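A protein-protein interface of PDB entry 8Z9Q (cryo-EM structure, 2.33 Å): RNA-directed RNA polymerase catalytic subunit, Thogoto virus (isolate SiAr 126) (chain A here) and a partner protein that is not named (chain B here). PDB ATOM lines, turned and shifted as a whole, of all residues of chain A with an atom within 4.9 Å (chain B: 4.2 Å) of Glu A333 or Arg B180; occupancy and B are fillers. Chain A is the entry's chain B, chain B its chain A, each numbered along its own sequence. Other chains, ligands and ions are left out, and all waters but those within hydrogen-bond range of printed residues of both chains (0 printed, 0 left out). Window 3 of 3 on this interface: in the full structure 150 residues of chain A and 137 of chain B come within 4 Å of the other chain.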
ATOM      1  N   GLU A 170      17.654  31.121 -11.020  1.00  0.00           N
ATOM      2  CA  GLU A 170      16.624  30.183 -11.441  1.00  0.00           C
ATOM      3  C   GLU A 170      15.390  30.209 -10.552  1.00  0.00           C
ATOM      4  O   GLU A 170      14.453  29.442 -10.796  1.00  0.00           O
ATOM      5  CB  GLU A 170      17.206  28.773 -11.476  1.00  0.00           C
ATOM      6  CG  GLU A 170      18.391  28.693 -12.400  1.00  0.00           C
ATOM      7  CD  GLU A 170      18.100  27.920 -13.654  1.00  0.00           C
ATOM      8  OE1 GLU A 170      19.060  27.640 -14.391  1.00  0.00           O
ATOM      9  OE2 GLU A 170      16.923  27.582 -13.895  1.00  0.00           O
ATOM     10  N   ASP A 329      32.393  20.772 -20.906  1.00  0.00           N
ATOM     11  CA  ASP A 329      31.333  21.688 -21.316  1.00  0.00           C
ATOM     12  C   ASP A 329      31.026  22.727 -20.246  1.00  0.00           C
ATOM     13  O   ASP A 329      30.616  23.846 -20.575  1.00  0.00           O
ATOM     14  CB  ASP A 329      30.070  20.907 -21.670  1.00  0.00           C
ATOM     15  CG  ASP A 329      30.148  20.265 -23.038  1.00  0.00           C
ATOM     16  OD1 ASP A 329      31.252  20.241 -23.621  1.00  0.00           O
ATOM     17  OD2 ASP A 329      29.107  19.786 -23.532  1.00  0.00           O
ATOM     18  N   TRP A 330      31.198  22.384 -18.967  1.00  0.00           N
ATOM     19  CA  TRP A 330      30.913  23.355 -17.916  1.00  0.00           C
ATOM     20  C   TRP A 330      31.919  24.501 -17.920  1.00  0.00           C
ATOM     21  O   TRP A 330      31.555  25.638 -17.603  1.00  0.00           O
ATOM     22  CB  TRP A 330      30.855  22.662 -16.553  1.00  0.00           C
ATOM     23  CG  TRP A 330      32.125  22.014 -16.094  1.00  0.00           C
ATOM     24  CD1 TRP A 330      32.535  20.744 -16.363  1.00  0.00           C
ATOM     25  CD2 TRP A 330      33.127  22.589 -15.248  1.00  0.00           C
ATOM     26  NE1 TRP A 330      33.741  20.499 -15.757  1.00  0.00           N
ATOM     27  CE2 TRP A 330      34.125  21.615 -15.063  1.00  0.00           C
ATOM     28  CE3 TRP A 330      33.281  23.836 -14.636  1.00  0.00           C
ATOM     29  CZ2 TRP A 330      35.262  21.849 -14.295  1.00  0.00           C
ATOM     30  CZ3 TRP A 330      34.407  24.065 -13.873  1.00  0.00           C
ATOM     31  CH2 TRP A 330      35.384  23.078 -13.710  1.00  0.00           C
ATOM     32  N   ILE A 331      33.168  24.234 -18.306  1.00  0.00           N
ATOM     33  CA  ILE A 331      34.129  25.316 -18.517  1.00  0.00           C
ATOM     34  C   ILE A 331      33.642  26.249 -19.621  1.00  0.00           C
ATOM     35  O   ILE A 331      33.713  27.479 -19.494  1.00  0.00           O
ATOM     36  CB  ILE A 331      35.519  24.738 -18.841  1.00  0.00           C
ATOM     37  CG1 ILE A 331      36.113  24.051 -17.615  1.00  0.00           C
ATOM     38  CG2 ILE A 331      36.453  25.831 -19.328  1.00  0.00           C
ATOM     39  CD1 ILE A 331      36.460  25.011 -16.505  1.00  0.00           C
ATOM     40  N   MET A 332      33.145  25.677 -20.719  1.00  0.00           N
ATOM     41  CA  MET A 332      32.636  26.485 -21.822  1.00  0.00           C
ATOM     42  C   MET A 332      31.467  27.346 -21.370  1.00  0.00           C
ATOM     43  O   MET A 332      31.394  28.537 -21.691  1.00  0.00           O
ATOM     44  CB  MET A 332      32.209  25.575 -22.971  1.00  0.00           C
ATOM     45  CG  MET A 332      33.345  24.839 -23.643  1.00  0.00           C
ATOM     46  SD  MET A 332      32.736  23.790 -24.972  1.00  0.00           S
ATOM     47  CE  MET A 332      34.251  23.001 -25.486  1.00  0.00           C
ATOM     48  N   GLU A 333      30.538  26.754 -20.617  1.00  0.00           N
ATOM     49  CA  GLU A 333      29.387  27.507 -20.130  1.00  0.00           C
ATOM     50  C   GLU A 333      29.825  28.631 -19.201  1.00  0.00           C
ATOM     51  O   GLU A 333      29.307  29.754 -19.281  1.00  0.00           O
ATOM     52  CB  GLU A 333      28.418  26.562 -19.419  1.00  0.00           C
ATOM     53  CG  GLU A 333      27.574  25.724 -20.365  1.00  0.00           C
ATOM     54  CD  GLU A 333      26.773  24.657 -19.648  1.00  0.00           C
ATOM     55  OE1 GLU A 333      27.390  23.755 -19.043  1.00  0.00           O
ATOM     56  OE2 GLU A 333      25.527  24.712 -19.697  1.00  0.00           O
ATOM     57  N   LEU A 334      30.782  28.345 -18.316  1.00  0.00           N
ATOM     58  CA  LEU A 334      31.293  29.362 -17.405  1.00  0.00           C
ATOM     59  C   LEU A 334      31.922  30.521 -18.164  1.00  0.00           C
ATOM     60  O   LEU A 334      31.723  31.687 -17.806  1.00  0.00           O
ATOM     61  CB  LEU A 334      32.309  28.733 -16.452  1.00  0.00           C
ATOM     62  CG  LEU A 334      32.827  29.592 -15.300  1.00  0.00           C
ATOM     63  CD1 LEU A 334      31.719  29.893 -14.305  1.00  0.00           C
ATOM     64  CD2 LEU A 334      34.000  28.907 -14.624  1.00  0.00           C
ATOM     65  N   PHE A 335      32.691  30.221 -19.213  1.00  0.00           N
ATOM     66  CA  PHE A 335      33.329  31.287 -19.978  1.00  0.00           C
ATOM     67  C   PHE A 335      32.336  32.042 -20.853  1.00  0.00           C
ATOM     68  O   PHE A 335      32.568  33.211 -21.178  1.00  0.00           O
ATOM     69  CB  PHE A 335      34.458  30.723 -20.835  1.00  0.00           C
ATOM     70  CG  PHE A 335      35.754  30.560 -20.099  1.00  0.00           C
ATOM     71  CD1 PHE A 335      35.837  29.752 -18.981  1.00  0.00           C
ATOM     72  CD2 PHE A 335      36.892  31.219 -20.529  1.00  0.00           C
ATOM     73  CE1 PHE A 335      37.029  29.604 -18.305  1.00  0.00           C
ATOM     74  CE2 PHE A 335      38.086  31.074 -19.858  1.00  0.00           C
ATOM     75  CZ  PHE A 335      38.156  30.265 -18.744  1.00  0.00           C
ATOM     76  N   ASN A 336      31.236  31.404 -21.248  1.00  0.00           N
ATOM     77  CA  ASN A 336      30.282  32.048 -22.141  1.00  0.00           C
ATOM     78  C   ASN A 336      29.215  32.858 -21.419  1.00  0.00           C
ATOM     79  O   ASN A 336      28.626  33.754 -22.034  1.00  0.00           O
ATOM     80  CB  ASN A 336      29.603  31.008 -23.033  1.00  0.00           C
ATOM     81  CG  ASN A 336      30.545  30.418 -24.063  1.00  0.00           C
ATOM     82  OD1 ASN A 336      30.593  29.205 -24.256  1.00  0.00           O
ATOM     83  ND2 ASN A 336      31.300  31.277 -24.734  1.00  0.00           N
ATOM     84  N   ILE A 337      28.938  32.564 -20.145  1.00  0.00           N
ATOM     85  CA  ILE A 337      27.954  33.358 -19.399  1.00  0.00           C
ATOM     86  C   ILE A 337      28.277  34.851 -19.386  1.00  0.00           C
ATOM     87  O   ILE A 337      27.365  35.657 -19.634  1.00  0.00           O
ATOM     88  CB  ILE A 337      27.774  32.787 -17.981  1.00  0.00           C
ATOM     89  CG1 ILE A 337      26.974  31.486 -18.018  1.00  0.00           C
ATOM     90  CG2 ILE A 337      27.089  33.798 -17.075  1.00  0.00           C
ATOM     91  CD1 ILE A 337      27.366  30.501 -16.944  1.00  0.00           C
ATOM     92  N   VAL B 175      24.436  24.912 -15.298  1.00  0.00           N
ATOM     93  CA  VAL B 175      23.510  25.963 -15.707  1.00  0.00           C
ATOM     94  C   VAL B 175      22.196  25.290 -16.075  1.00  0.00           C
ATOM     95  O   VAL B 175      22.163  24.427 -16.962  1.00  0.00           O
ATOM     96  CB  VAL B 175      24.055  26.782 -16.887  1.00  0.00           C
ATOM     97  CG1 VAL B 175      23.032  27.811 -17.335  1.00  0.00           C
ATOM     98  CG2 VAL B 175      25.356  27.454 -16.506  1.00  0.00           C
ATOM     99  N   GLY B 176      21.118  25.679 -15.399  1.00  0.00           N
ATOM    100  CA  GLY B 176      19.828  25.069 -15.624  1.00  0.00           C
ATOM    101  C   GLY B 176      19.078  25.695 -16.783  1.00  0.00           C
ATOM    102  O   GLY B 176      19.599  26.507 -17.544  1.00  0.00           O
ATOM    103  N   THR B 177      17.807  25.302 -16.904  1.00  0.00           N
ATOM    104  CA  THR B 177      17.028  25.656 -18.087  1.00  0.00           C
ATOM    105  C   THR B 177      16.646  27.132 -18.104  1.00  0.00           C
ATOM    106  O   THR B 177      16.763  27.794 -19.142  1.00  0.00           O
ATOM    107  CB  THR B 177      15.774  24.787 -18.164  1.00  0.00           C
ATOM    108  OG1 THR B 177      15.111  24.789 -16.894  1.00  0.00           O
ATOM    109  CG2 THR B 177      16.141  23.358 -18.530  1.00  0.00           C
ATOM    110  N   THR B 178      16.181  27.667 -16.973  1.00  0.00           N
ATOM    111  CA  THR B 178      15.610  29.011 -16.980  1.00  0.00           C
ATOM    112  C   THR B 178      16.683  30.078 -17.167  1.00  0.00           C
ATOM    113  O   THR B 178      16.501  31.024 -17.946  1.00  0.00           O
ATOM    114  CB  THR B 178      14.829  29.255 -15.692  1.00  0.00           C
ATOM    115  OG1 THR B 178      13.978  28.134 -15.433  1.00  0.00           O
ATOM    116  CG2 THR B 178      13.970  30.486 -15.837  1.00  0.00           C
ATOM    117  N   PHE B 179      17.804  29.952 -16.454  1.00  0.00           N
ATOM    118  CA  PHE B 179      18.914  30.872 -16.669  1.00  0.00           C
ATOM    119  C   PHE B 179      19.459  30.746 -18.084  1.00  0.00           C
ATOM    120  O   PHE B 179      19.894  31.741 -18.674  1.00  0.00           O
ATOM    121  CB  PHE B 179      20.011  30.615 -15.635  1.00  0.00           C
ATOM    122  CG  PHE B 179      21.125  31.623 -15.661  1.00  0.00           C
ATOM    123  CD1 PHE B 179      20.852  32.974 -15.784  1.00  0.00           C
ATOM    124  CD2 PHE B 179      22.443  31.219 -15.542  1.00  0.00           C
ATOM    125  CE1 PHE B 179      21.874  33.901 -15.803  1.00  0.00           C
ATOM    126  CE2 PHE B 179      23.468  32.143 -15.556  1.00  0.00           C
ATOM    127  CZ  PHE B 179      23.183  33.485 -15.688  1.00  0.00           C
ATOM    128  N   ARG B 180      19.426  29.538 -18.649  1.00  0.00           N
ATOM    129  CA  ARG B 180      19.832  29.347 -20.036  1.00  0.00           C
ATOM    130  C   ARG B 180      18.921  30.111 -20.992  1.00  0.00           C
ATOM    131  O   ARG B 180      19.394  30.747 -21.942  1.00  0.00           O
ATOM    132  CB  ARG B 180      19.836  27.856 -20.365  1.00  0.00           C
ATOM    133  CG  ARG B 180      20.545  27.492 -21.644  1.00  0.00           C
ATOM    134  CD  ARG B 180      20.689  25.987 -21.774  1.00  0.00           C
ATOM    135  NE  ARG B 180      21.363  25.405 -20.621  1.00  0.00           N
ATOM    136  CZ  ARG B 180      22.602  24.931 -20.639  1.00  0.00           C
ATOM    137  NH1 ARG B 180      23.335  24.955 -21.738  1.00  0.00           N
ATOM    138  NH2 ARG B 180      23.117  24.421 -19.525  1.00  0.00           N
ATOM    139  N   THR B 181      17.608  30.056 -20.756  1.00  0.00           N
ATOM    140  CA  THR B 181      16.675  30.799 -21.600  1.00  0.00           C
ATOM    141  C   THR B 181      16.877  32.301 -21.454  1.00  0.00           C
ATOM    142  O   THR B 181      16.781  33.042 -22.439  1.00  0.00           O
ATOM    143  CB  THR B 181      15.233  30.420 -21.265  1.00  0.00           C
ATOM    144  OG1 THR B 181      14.968  30.702 -19.886  1.00  0.00           O
ATOM    145  CG2 THR B 181      14.990  28.946 -21.538  1.00  0.00           C
ATOM    146  N   LEU B 182      17.140  32.772 -20.232  1.00  0.00           N
ATOM    147  CA  LEU B 182      17.446  34.188 -20.046  1.00  0.00           C
ATOM    148  C   LEU B 182      18.706  34.580 -20.806  1.00  0.00           C
ATOM    149  O   LEU B 182      18.764  35.650 -21.423  1.00  0.00           O
ATOM    150  CB  LEU B 182      17.604  34.514 -18.562  1.00  0.00           C
ATOM    151  CG  LEU B 182      16.363  34.460 -17.673  1.00  0.00           C
ATOM    152  CD1 LEU B 182      16.752  34.684 -16.225  1.00  0.00           C
ATOM    153  CD2 LEU B 182      15.350  35.491 -18.115  1.00  0.00           C
ATOM    154  N   LEU B 183      19.729  33.726 -20.766  1.00  0.00           N
ATOM    155  CA  LEU B 183      20.982  34.018 -21.452  1.00  0.00           C
ATOM    156  C   LEU B 183      20.796  34.058 -22.964  1.00  0.00           C
ATOM    157  O   LEU B 183      21.393  34.899 -23.646  1.00  0.00           O
ATOM    158  CB  LEU B 183      22.030  32.975 -21.066  1.00  0.00           C
ATOM    159  CG  LEU B 183      22.724  33.149 -19.716  1.00  0.00           C
ATOM    160  CD1 LEU B 183      23.555  31.921 -19.391  1.00  0.00           C
ATOM    161  CD2 LEU B 183      23.585  34.394 -19.715  1.00  0.00           C
ATOM    162  N   LYS B 184      19.981  33.156 -23.506  1.00  0.00           N
ATOM    163  CA  LYS B 184      19.774  33.057 -24.947  1.00  0.00           C
ATOM    164  C   LYS B 184      18.890  34.163 -25.515  1.00  0.00           C
ATOM    165  O   LYS B 184      18.576  34.122 -26.710  1.00  0.00           O
ATOM    166  CB  LYS B 184      19.161  31.697 -25.297  1.00  0.00           C
ATOM    167  CG  LYS B 184      20.133  30.533 -25.289  1.00  0.00           C
ATOM    168  CD  LYS B 184      19.422  29.252 -25.693  1.00  0.00           C
ATOM    169  CE  LYS B 184      20.401  28.131 -25.992  1.00  0.00           C
ATOM    170  NZ  LYS B 184      21.173  27.704 -24.798  1.00  0.00           N
ATOM    171  N   VAL B 191      24.345  28.641 -25.597  1.00  0.00           N
ATOM    172  CA  VAL B 191      25.298  28.975 -24.541  1.00  0.00           C
ATOM    173  C   VAL B 191      26.713  28.653 -24.997  1.00  0.00           C
ATOM    174  O   VAL B 191      27.637  29.457 -24.834  1.00  0.00           O
ATOM    175  CB  VAL B 191      24.939  28.246 -23.235  1.00  0.00           C
ATOM    176  CG1 VAL B 191      26.075  28.365 -22.240  1.00  0.00           C
ATOM    177  CG2 VAL B 191      23.672  28.824 -22.647  1.00  0.00           C
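The side-chain hydroxyl (OG1) of Thr B181 lies close to the backbone carbonyl oxygen (O) of Thr B177 (3.5 Å).
The side-chain amide oxygen (OD1) of Asn A336 sits close to the backbone carbonyl oxygen (O) of Met A332 (2.8 Å).
The backbone carbonyl oxygen (O) of Val B175 is in hydrogen-bond range of the guanidinium group (NH2) of Arg B180, at 2.7 Å.
O of Thr B178 lies within hydrogen-bond range of OG1 of Thr B181, 2.5 Å away.
Glu A333 touches just these residues of chain B: Val B175 (3.8 Å), Arg B180 (2.4 Å) and Val B191 (3.6 Å).
Of chain A, only Glu A333 (2.4 Å) comes within 4 Å of Arg B180.
Of the printed residues of chain A, Leu B183 touches Ile A337.
Of the printed residues of chain A, Thr B177 touches Glu A170.
Of the printed residues of chain B, Asn A336 touches Val B191 (3.0 Å).
Asp A329 touches none of the printed residues of chain B.
Thr B181 touches none of the printed residues of chain A.
The nearest printed residue of chain B that does not touch Glu A333 is Leu B183 (6.1 Å).
The nearest printed residue of chain A that does not touch Phe B179 is Ile A337 (4.2 Å).
The side-chain carboxylate of Glu A333 is in salt-bridge range of the guanidinium group of Arg B180 (2.4 Å).
The side-chain carboxylate (OE2) of Glu A170 sits at hydrogen-bond distance from the backbone NH (N) of Thr B178 (3.2 Å).
OE1 of Glu A170 lies close to N of Gly B176.
OE1 of Glu A170 is in hydrogen-bond range of N of Phe B179 (3.3 Å).
The side-chain amide oxygen (OD1) of Asn A336 sits close to the backbone carbonyl oxygen (O) of Val B191.
Hydrophobic or aromatic side chains of chain B within 4 Å of the printed part of chain A: Val B175, Phe B179, Leu B183 and Val B191.
Of the 10 printed residues of chain A, 4 touch a printed residue of chain B.
Printed residues of chain A that touch a printed residue of chain B: Glu A170, Glu A333, Asn A336 and Ile A337.
Hydrophobic or aromatic side chains of chain A that line the printed part of chain B: Ile A337.
Among the printed residues, pairs that only touch across the chains: Glu A333 with Val B191 (3.6 Å), Glu A170 with Thr B177 (3.7 Å), Ile A337 with Val B175 (3.7 Å), Ile A337 with Leu B183 (3.7 Å) and Glu A333 with Val B175 (3.8 Å).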
